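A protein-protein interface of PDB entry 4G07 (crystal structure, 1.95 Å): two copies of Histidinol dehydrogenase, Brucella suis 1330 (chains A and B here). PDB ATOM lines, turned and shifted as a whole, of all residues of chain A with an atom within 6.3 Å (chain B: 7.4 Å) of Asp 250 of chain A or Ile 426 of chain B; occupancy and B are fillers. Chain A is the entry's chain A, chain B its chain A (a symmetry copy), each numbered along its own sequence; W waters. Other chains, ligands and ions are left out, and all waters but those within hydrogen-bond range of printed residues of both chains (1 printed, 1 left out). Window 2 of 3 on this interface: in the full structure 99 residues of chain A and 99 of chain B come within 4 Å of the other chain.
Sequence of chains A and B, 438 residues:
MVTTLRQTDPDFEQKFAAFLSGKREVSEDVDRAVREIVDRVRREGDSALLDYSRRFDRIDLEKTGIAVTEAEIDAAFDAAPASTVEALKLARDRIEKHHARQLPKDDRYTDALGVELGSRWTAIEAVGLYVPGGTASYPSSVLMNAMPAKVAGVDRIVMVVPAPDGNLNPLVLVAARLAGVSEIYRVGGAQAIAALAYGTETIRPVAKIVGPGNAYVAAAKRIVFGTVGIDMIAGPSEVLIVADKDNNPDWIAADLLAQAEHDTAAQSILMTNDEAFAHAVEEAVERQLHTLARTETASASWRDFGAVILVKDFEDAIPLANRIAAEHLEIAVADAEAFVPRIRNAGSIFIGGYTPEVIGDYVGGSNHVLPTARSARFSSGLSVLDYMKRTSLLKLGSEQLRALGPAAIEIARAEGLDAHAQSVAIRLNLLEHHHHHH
The indole nitrogen of Trp 251 of chain A sits at hydrogen-bond distance from the backbone carbonyl oxygen of Ile 426 of chain B (3.5 Å). The side-chain carboxylate (OD2) of Asp 255 of chain A lies within salt-bridge range of the guanidinium group (NH2) of Arg 427 of chain B (2.7 Å).
The side-chain amide oxygen (OD1) of Asn 248 of chain A lies within hydrogen-bond range of the backbone NH (N) of Asp 250 of chain A, 2.9 Å away. NE1 of Trp 251 of chain A sits close to ND2 of Asn 248 of chain A, at 3.2 Å. The guanidinium group of Arg 287 of chain A is in salt-bridge range of the side-chain carboxylate of Asp 250 of chain A (2.8 Å). The backbone carbonyl oxygen (O) of Asp 250 of chain A sits at hydrogen-bond distance from the side-chain amide nitrogen (NE2) of Gln 288 of chain A, at 2.8 Å. The side-chain amide oxygen (OE1) of Gln 288 of chain A sits at hydrogen-bond distance from the backbone NH (N) of Ala 254 of chain A. The backbone carbonyl oxygen of Ser 423 of chain B is in hydrogen-bond range of the guanidinium group of Arg 427 of chain B, 2.6 Å away.
Among the printed residues, pairs that only touch across the chains: Asp 250 of chain A with Ile 426 of chain B, Trp 251 of chain A with Arg 427 of chain B, Ala 254 of chain A with Ser 423 of chain B, Asp 255 of chain A with Ser 423 of chain B and Gln 288 of chain A with Ile 426 of chain B.
Printed residues of chain A within 4 Å of Arg 427 of chain B: Trp 251 and Asp 255. Printed residues of chain B within 4 Å of Trp 251 of chain A: Ile 426 (3.5 Å) and Arg 427 (3.7 Å). Of the printed residues of chain B, Gln 288 of chain A touches Ile 426 (3.7 Å). Ala 425 of chain B touches none of the printed residues of chain A. Asn 429 of chain B touches none of the printed residues of chain A. The nearest residue of chain A that does not touch Ile 426 of chain B is Ala 254 of chain A (4.2 Å). The nearest printed residue of chain A that does not touch Ser 423 of chain B is Trp 251 of chain A (5.5 Å).
Of the 14 printed residues of chain A, 5 touch a printed residue of chain B. Hydrophobic or aromatic side chains of chain A that line the printed part of chain B: Trp 251 and Ala 254. Of the 14 printed residues of chain B, 3 touch a printed residue of chain A. Hydrophobic or aromatic side chains of chain B that line the printed part of chain A: Ile 426. Along chain B the printed residues that touch a printed residue of chain A span positions 423 to 427. Among the printed residues, Asp or Glu carboxylates within 4 Å of a Lys or Arg side-chain nitrogen of the other chain: Asp 255 of chain A with Arg 427 of chain B.
No position is printed for both chains. Of the 7 pairs that touch across the chains among the printed residues, none has its exchanged pair printed and touching as well.
Water W1 lies within hydrogen-bond range of the side-chain hydroxyl of Ser 423 of chain B (3.3 Å) and the side-chain carboxylate of Asp 255 of chain A (3.3 Å).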
ATOM      1  N   ASN A 247       4.121 -19.595  -7.997  1.00  0.00           N
ATOM      2  CA  ASN A 247       3.863 -20.437  -6.832  1.00  0.00           C
ATOM      3  C   ASN A 247       2.595 -19.942  -6.180  1.00  0.00           C
ATOM      4  O   ASN A 247       2.152 -18.834  -6.440  1.00  0.00           O
ATOM      5  CB  ASN A 247       5.001 -20.333  -5.802  1.00  0.00           C
ATOM      6  CG  ASN A 247       6.277 -20.985  -6.279  1.00  0.00           C
ATOM      7  OD1 ASN A 247       7.177 -20.324  -6.818  1.00  0.00           O
ATOM      8  ND2 ASN A 247       6.361 -22.293  -6.106  1.00  0.00           N
ATOM      9  N   ASN A 248       2.020 -20.771  -5.327  1.00  0.00           N
ATOM     10  CA  ASN A 248       0.831 -20.407  -4.590  1.00  0.00           C
ATOM     11  C   ASN A 248       1.350 -19.675  -3.351  1.00  0.00           C
ATOM     12  O   ASN A 248       2.039 -20.262  -2.510  1.00  0.00           O
ATOM     13  CB  ASN A 248       0.070 -21.665  -4.180  1.00  0.00           C
ATOM     14  CG  ASN A 248      -1.205 -21.353  -3.444  1.00  0.00           C
ATOM     15  OD1 ASN A 248      -1.314 -20.329  -2.769  1.00  0.00           O
ATOM     16  ND2 ASN A 248      -2.175 -22.246  -3.549  1.00  0.00           N
ATOM     17  N   PRO A 249       1.023 -18.381  -3.220  1.00  0.00           N
ATOM     18  CA  PRO A 249       1.464 -17.573  -2.078  1.00  0.00           C
ATOM     19  C   PRO A 249       1.087 -18.170  -0.721  1.00  0.00           C
ATOM     20  O   PRO A 249       1.847 -18.046   0.230  1.00  0.00           O
ATOM     21  CB  PRO A 249       0.787 -16.220  -2.315  1.00  0.00           C
ATOM     22  CG  PRO A 249       0.547 -16.186  -3.793  1.00  0.00           C
ATOM     23  CD  PRO A 249       0.147 -17.606  -4.116  1.00  0.00           C
ATOM     24  N   ASP A 250      -0.088 -18.798  -0.633  1.00  0.00           N
ATOM     25  CA  ASP A 250      -0.554 -19.412   0.622  1.00  0.00           C
ATOM     26  C   ASP A 250       0.332 -20.578   1.039  1.00  0.00           C
ATOM     27  O   ASP A 250       0.565 -20.804   2.229  1.00  0.00           O
ATOM     28  CB  ASP A 250      -1.985 -19.957   0.489  1.00  0.00           C
ATOM     29  CG  ASP A 250      -3.003 -18.891   0.153  1.00  0.00           C
ATOM     30  OD1 ASP A 250      -3.002 -17.830   0.801  1.00  0.00           O
ATOM     31  OD2 ASP A 250      -3.821 -19.140  -0.757  1.00  0.00           O
ATOM     32  N   TRP A 251       0.784 -21.334   0.045  1.00  0.00           N
ATOM     33  CA  TRP A 251       1.651 -22.480   0.261  1.00  0.00           C
ATOM     34  C   TRP A 251       3.010 -22.025   0.807  1.00  0.00           C
ATOM     35  O   TRP A 251       3.534 -22.590   1.774  1.00  0.00           O
ATOM     36  CB  TRP A 251       1.835 -23.215  -1.058  1.00  0.00           C
ATOM     37  CG  TRP A 251       0.627 -23.987  -1.467  1.00  0.00           C
ATOM     38  CD1 TRP A 251      -0.658 -23.819  -1.008  1.00  0.00           C
ATOM     39  CD2 TRP A 251       0.581 -25.058  -2.411  1.00  0.00           C
ATOM     40  NE1 TRP A 251      -1.499 -24.728  -1.614  1.00  0.00           N
ATOM     41  CE2 TRP A 251      -0.764 -25.500  -2.479  1.00  0.00           C
ATOM     42  CE3 TRP A 251       1.546 -25.690  -3.210  1.00  0.00           C
ATOM     43  CZ2 TRP A 251      -1.166 -26.545  -3.311  1.00  0.00           C
ATOM     44  CZ3 TRP A 251       1.147 -26.733  -4.040  1.00  0.00           C
ATOM     45  CH2 TRP A 251      -0.202 -27.149  -4.082  1.00  0.00           C
ATOM     46  N   ILE A 252       3.568 -20.994   0.182  1.00  0.00           N
ATOM     47  CA  ILE A 252       4.858 -20.457   0.599  1.00  0.00           C
ATOM     48  C   ILE A 252       4.741 -19.880   2.014  1.00  0.00           C
ATOM     49  O   ILE A 252       5.639 -20.045   2.845  1.00  0.00           O
ATOM     50  CB  ILE A 252       5.348 -19.379  -0.415  1.00  0.00           C
ATOM     51  CG1 ILE A 252       5.559 -20.033  -1.787  1.00  0.00           C
ATOM     52  CG2 ILE A 252       6.639 -18.716   0.075  1.00  0.00           C
ATOM     53  CD1 ILE A 252       6.539 -21.193  -1.814  1.00  0.00           C
ATOM     54  N   ALA A 253       3.621 -19.222   2.296  1.00  0.00           N
ATOM     55  CA  ALA A 253       3.394 -18.648   3.615  1.00  0.00           C
ATOM     56  C   ALA A 253       3.319 -19.768   4.660  1.00  0.00           C
ATOM     57  O   ALA A 253       3.924 -19.678   5.726  1.00  0.00           O
ATOM     58  CB  ALA A 253       2.084 -17.820   3.618  1.00  0.00           C
ATOM     59  N   ALA A 254       2.584 -20.828   4.341  1.00  0.00           N
ATOM     60  CA  ALA A 254       2.450 -21.952   5.259  1.00  0.00           C
ATOM     61  C   ALA A 254       3.829 -22.524   5.591  1.00  0.00           C
ATOM     62  O   ALA A 254       4.099 -22.909   6.731  1.00  0.00           O
ATOM     63  CB  ALA A 254       1.570 -23.031   4.642  1.00  0.00           C
ATOM     64  N   ASP A 255       4.703 -22.575   4.592  1.00  0.00           N
ATOM     65  CA  ASP A 255       6.038 -23.107   4.809  1.00  0.00           C
ATOM     66  C   ASP A 255       6.858 -22.216   5.728  1.00  0.00           C
ATOM     67  O   ASP A 255       7.605 -22.711   6.572  1.00  0.00           O
ATOM     68  CB  ASP A 255       6.754 -23.304   3.467  1.00  0.00           C
ATOM     69  CG  ASP A 255       6.109 -24.386   2.614  1.00  0.00           C
ATOM     70  OD1 ASP A 255       5.263 -25.144   3.136  1.00  0.00           O
ATOM     71  OD2 ASP A 255       6.449 -24.494   1.419  1.00  0.00           O
ATOM     72  N   ALA A 280       2.296 -10.627  -1.789  1.00  0.00           N
ATOM     73  CA  ALA A 280       1.244 -11.625  -1.752  1.00  0.00           C
ATOM     74  C   ALA A 280       1.549 -12.712  -0.712  1.00  0.00           C
ATOM     75  O   ALA A 280       0.638 -13.297  -0.133  1.00  0.00           O
ATOM     76  CB  ALA A 280       1.066 -12.247  -3.136  1.00  0.00           C
ATOM     77  N   VAL A 281       2.825 -12.996  -0.479  1.00  0.00           N
ATOM     78  CA  VAL A 281       3.172 -14.010   0.506  1.00  0.00           C
ATOM     79  C   VAL A 281       2.986 -13.436   1.915  1.00  0.00           C
ATOM     80  O   VAL A 281       2.500 -14.125   2.811  1.00  0.00           O
ATOM     81  CB  VAL A 281       4.637 -14.519   0.315  1.00  0.00           C
ATOM     82  CG1 VAL A 281       5.008 -15.499   1.424  1.00  0.00           C
ATOM     83  CG2 VAL A 281       4.778 -15.196  -1.050  1.00  0.00           C
ATOM     84  N   ALA A 284      -0.576 -13.518   2.929  1.00  0.00           N
ATOM     85  CA  ALA A 284      -0.999 -14.873   3.238  1.00  0.00           C
ATOM     86  C   ALA A 284      -0.476 -15.255   4.631  1.00  0.00           C
ATOM     87  O   ALA A 284      -1.173 -15.923   5.402  1.00  0.00           O
ATOM     88  CB  ALA A 284      -0.475 -15.841   2.190  1.00  0.00           C
ATOM     89  N   ARG A 287      -2.921 -13.668   7.173  1.00  0.00           N
ATOM     90  CA  ARG A 287      -4.218 -14.322   7.282  1.00  0.00           C
ATOM     91  C   ARG A 287      -4.129 -15.674   7.991  1.00  0.00           C
ATOM     92  O   ARG A 287      -4.966 -15.997   8.834  1.00  0.00           O
ATOM     93  CB  ARG A 287      -4.829 -14.507   5.894  1.00  0.00           C
ATOM     94  CG  ARG A 287      -5.410 -13.240   5.287  1.00  0.00           C
ATOM     95  CD  ARG A 287      -5.388 -13.323   3.775  1.00  0.00           C
ATOM     96  NE  ARG A 287      -5.600 -14.692   3.329  1.00  0.00           N
ATOM     97  CZ  ARG A 287      -4.993 -15.236   2.280  1.00  0.00           C
ATOM     98  NH1 ARG A 287      -4.135 -14.522   1.560  1.00  0.00           N
ATOM     99  NH2 ARG A 287      -5.226 -16.507   1.967  1.00  0.00           N
ATOM    100  N   GLN A 288      -3.116 -16.463   7.644  1.00  0.00           N
ATOM    101  CA  GLN A 288      -2.940 -17.777   8.251  1.00  0.00           C
ATOM    102  C   GLN A 288      -2.531 -17.648   9.703  1.00  0.00           C
ATOM    103  O   GLN A 288      -2.807 -18.531  10.509  1.00  0.00           O
ATOM    104  CB  GLN A 288      -1.870 -18.573   7.509  1.00  0.00           C
ATOM    105  CG  GLN A 288      -2.295 -19.114   6.160  1.00  0.00           C
ATOM    106  CD  GLN A 288      -1.125 -19.701   5.396  1.00  0.00           C
ATOM    107  OE1 GLN A 288      -0.098 -20.054   5.986  1.00  0.00           O
ATOM    108  NE2 GLN A 288      -1.272 -19.818   4.083  1.00  0.00           N
ATOM    109  N   LEU B 401       3.379 -36.703  -2.420  1.00  0.00           N
ATOM    110  CA  LEU B 401       2.876 -35.957  -1.275  1.00  0.00           C
ATOM    111  C   LEU B 401       1.536 -36.552  -0.842  1.00  0.00           C
ATOM    112  O   LEU B 401       1.219 -36.620   0.353  1.00  0.00           O
ATOM    113  CB  LEU B 401       2.693 -34.479  -1.620  1.00  0.00           C
ATOM    114  CG  LEU B 401       2.263 -33.693  -0.390  1.00  0.00           C
ATOM    115  CD1 LEU B 401       3.423 -33.646   0.588  1.00  0.00           C
ATOM    116  CD2 LEU B 401       1.840 -32.287  -0.773  1.00  0.00           C
ATOM    117  N   ILE B 409       1.170 -35.427   8.565  1.00  0.00           N
ATOM    118  CA  ILE B 409       0.172 -34.649   9.283  1.00  0.00           C
ATOM    119  C   ILE B 409      -0.130 -35.301  10.636  1.00  0.00           C
ATOM    120  O   ILE B 409      -0.178 -34.630  11.676  1.00  0.00           O
ATOM    121  CB  ILE B 409      -1.123 -34.538   8.430  1.00  0.00           C
ATOM    122  CG1 ILE B 409      -0.857 -33.655   7.203  1.00  0.00           C
ATOM    123  CG2 ILE B 409      -2.256 -33.956   9.266  1.00  0.00           C
ATOM    124  CD1 ILE B 409      -2.035 -33.531   6.261  1.00  0.00           C
ATOM    125  N   ARG B 413       0.598 -33.347  14.119  1.00  0.00           N
ATOM    126  CA  ARG B 413      -0.476 -33.044  15.046  1.00  0.00           C
ATOM    127  C   ARG B 413      -0.261 -33.751  16.378  1.00  0.00           C
ATOM    128  O   ARG B 413      -0.567 -33.189  17.415  1.00  0.00           O
ATOM    129  CB  ARG B 413      -1.829 -33.390  14.433  1.00  0.00           C
ATOM    130  CG  ARG B 413      -2.340 -32.237  13.572  1.00  0.00           C
ATOM    131  CD  ARG B 413      -3.572 -32.590  12.784  1.00  0.00           C
ATOM    132  NE  ARG B 413      -3.879 -31.546  11.817  1.00  0.00           N
ATOM    133  CZ  ARG B 413      -4.641 -31.721  10.742  1.00  0.00           C
ATOM    134  NH1 ARG B 413      -5.188 -32.912  10.489  1.00  0.00           N
ATOM    135  NH2 ARG B 413      -4.842 -30.706   9.905  1.00  0.00           N
ATOM    136  N   ALA B 421       1.713 -29.246  10.308  1.00  0.00           N
ATOM    137  CA  ALA B 421       0.643 -30.053   9.726  1.00  0.00           C
ATOM    138  C   ALA B 421      -0.050 -29.282   8.605  1.00  0.00           C
ATOM    139  O   ALA B 421      -0.365 -29.847   7.553  1.00  0.00           O
ATOM    140  CB  ALA B 421      -0.369 -30.437  10.807  1.00  0.00           C
ATOM    141  N   GLN B 422      -0.277 -27.992   8.825  1.00  0.00           N
ATOM    142  CA  GLN B 422      -0.947 -27.171   7.816  1.00  0.00           C
ATOM    143  C   GLN B 422      -0.191 -27.002   6.493  1.00  0.00           C
ATOM    144  O   GLN B 422      -0.815 -26.935   5.434  1.00  0.00           O
ATOM    145  CB  GLN B 422      -1.282 -25.796   8.388  1.00  0.00           C
ATOM    146  CG  GLN B 422      -2.598 -25.788   9.147  1.00  0.00           C
ATOM    147  CD  GLN B 422      -3.720 -26.437   8.343  1.00  0.00           C
ATOM    148  OE1 GLN B 422      -4.062 -25.978   7.247  1.00  0.00           O
ATOM    149  NE2 GLN B 422      -4.285 -27.517   8.878  1.00  0.00           N
ATOM    150  N   SER B 423       1.137 -26.936   6.538  1.00  0.00           N
ATOM    151  CA  SER B 423       1.897 -26.784   5.297  1.00  0.00           C
ATOM    152  C   SER B 423       1.681 -28.006   4.385  1.00  0.00           C
ATOM    153  O   SER B 423       1.866 -27.923   3.163  1.00  0.00           O
ATOM    154  CB  SER B 423       3.395 -26.571   5.593  1.00  0.00           C
ATOM    155  OG  SER B 423       3.976 -27.734   6.148  1.00  0.00           O
ATOM    156  N   VAL B 424       1.293 -29.143   4.967  1.00  0.00           N
ATOM    157  CA  VAL B 424       1.009 -30.330   4.163  1.00  0.00           C
ATOM    158  C   VAL B 424      -0.484 -30.323   3.810  1.00  0.00           C
ATOM    159  O   VAL B 424      -0.866 -30.509   2.653  1.00  0.00           O
ATOM    160  CB  VAL B 424       1.330 -31.649   4.914  1.00  0.00           C
ATOM    161  CG1 VAL B 424       0.967 -32.844   4.027  1.00  0.00           C
ATOM    162  CG2 VAL B 424       2.812 -31.712   5.274  1.00  0.00           C
ATOM    163  N   ALA B 425      -1.324 -30.088   4.814  1.00  0.00           N
ATOM    164  CA  ALA B 425      -2.768 -30.070   4.606  1.00  0.00           C
ATOM    165  C   ALA B 425      -3.223 -29.050   3.544  1.00  0.00           C
ATOM    166  O   ALA B 425      -4.122 -29.342   2.753  1.00  0.00           O
ATOM    167  CB  ALA B 425      -3.489 -29.802   5.945  1.00  0.00           C
ATOM    168  N   ILE B 426      -2.602 -27.871   3.509  1.00  0.00           N
ATOM    169  CA  ILE B 426      -3.002 -26.841   2.548  1.00  0.00           C
ATOM    170  C   ILE B 426      -2.796 -27.314   1.111  1.00  0.00           C
ATOM    171  O   ILE B 426      -3.500 -26.881   0.193  1.00  0.00           O
ATOM    172  CB  ILE B 426      -2.242 -25.506   2.796  1.00  0.00           C
ATOM    173  CG1 ILE B 426      -2.943 -24.358   2.064  1.00  0.00           C
ATOM    174  CG2 ILE B 426      -0.816 -25.586   2.278  1.00  0.00           C
ATOM    175  CD1 ILE B 426      -2.485 -23.004   2.531  1.00  0.00           C
ATOM    176  N   ARG B 427      -1.839 -28.216   0.925  1.00  0.00           N
ATOM    177  CA  ARG B 427      -1.543 -28.767  -0.389  1.00  0.00           C
ATOM    178  C   ARG B 427      -2.455 -29.963  -0.673  1.00  0.00           C
ATOM    179  O   ARG B 427      -3.001 -30.090  -1.769  1.00  0.00           O
ATOM    180  CB  ARG B 427      -0.074 -29.218  -0.461  1.00  0.00           C
ATOM    181  CG  ARG B 427       0.940 -28.084  -0.282  1.00  0.00           C
ATOM    182  CD  ARG B 427       2.377 -28.620  -0.233  1.00  0.00           C
ATOM    183  NE  ARG B 427       3.363 -27.591  -0.579  1.00  0.00           N
ATOM    184  CZ  ARG B 427       3.819 -26.656   0.250  1.00  0.00           C
ATOM    185  NH1 ARG B 427       3.391 -26.592   1.504  1.00  0.00           N
ATOM    186  NH2 ARG B 427       4.727 -25.786  -0.178  1.00  0.00           N
ATOM    187  N   LEU B 428      -2.618 -30.842   0.313  1.00  0.00           N
ATOM    188  CA  LEU B 428      -3.466 -32.010   0.110  1.00  0.00           C
ATOM    189  C   LEU B 428      -4.930 -31.641  -0.096  1.00  0.00           C
ATOM    190  O   LEU B 428      -5.631 -32.293  -0.871  1.00  0.00           O
ATOM    191  CB  LEU B 428      -3.361 -32.978   1.288  1.00  0.00           C
ATOM    192  CG  LEU B 428      -2.042 -33.711   1.493  1.00  0.00           C
ATOM    193  CD1 LEU B 428      -2.214 -34.691   2.640  1.00  0.00           C
ATOM    194  CD2 LEU B 428      -1.634 -34.443   0.218  1.00  0.00           C
ATOM    195  N   ASN B 429      -5.386 -30.603   0.597  1.00  0.00           N
ATOM    196  CA  ASN B 429      -6.776 -30.168   0.489  1.00  0.00           C
ATOM    197  C   ASN B 429      -7.174 -29.796  -0.929  1.00  0.00           C
ATOM    198  O   ASN B 429      -8.311 -30.045  -1.341  1.00  0.00           O
ATOM    199  CB  ASN B 429      -7.052 -29.003   1.442  1.00  0.00           C
ATOM    200  CG  ASN B 429      -7.106 -29.451   2.889  1.00  0.00           C
ATOM    201  OD1 ASN B 429      -7.262 -30.644   3.165  1.00  0.00           O
ATOM    202  ND2 ASN B 429      -6.994 -28.504   3.821  1.00  0.00           N
ATOM    203  N   LEU B 430      -6.254 -29.197  -1.676  1.00  0.00           N
ATOM    204  CA  LEU B 430      -6.549 -28.840  -3.058  1.00  0.00           C
ATOM    205  C   LEU B 430      -6.354 -30.042  -3.979  1.00  0.00           C
ATOM    206  O   LEU B 430      -7.168 -30.310  -4.857  1.00  0.00           O
ATOM    207  CB  LEU B 430      -5.646 -27.694  -3.532  1.00  0.00           C
ATOM    208  CG  LEU B 430      -5.912 -26.323  -2.915  1.00  0.00           C
ATOM    209  CD1 LEU B 430      -5.057 -25.270  -3.623  1.00  0.00           C
ATOM    210  CD2 LEU B 430      -7.395 -25.990  -3.042  1.00  0.00           C
ATOM    211  N   LEU B 431      -5.265 -30.767  -3.750  1.00  0.00           N
ATOM    212  CA  LEU B 431      -4.896 -31.929  -4.543  1.00  0.00           C
ATOM    213  C   LEU B 431      -5.922 -33.067  -4.501  1.00  0.00           C
ATOM    214  O   LEU B 431      -6.155 -33.736  -5.507  1.00  0.00           O
ATOM    215  CB  LEU B 431      -3.541 -32.441  -4.041  1.00  0.00           C
ATOM    216  CG  LEU B 431      -2.693 -33.368  -4.910  1.00  0.00           C
ATOM    217  CD1 LEU B 431      -2.244 -32.646  -6.180  1.00  0.00           C
ATOM    218  CD2 LEU B 431      -1.476 -33.815  -4.104  1.00  0.00           C
HETATM  219  O   HOH W   1       7.042 -26.818   5.393  1.00  0.00           O
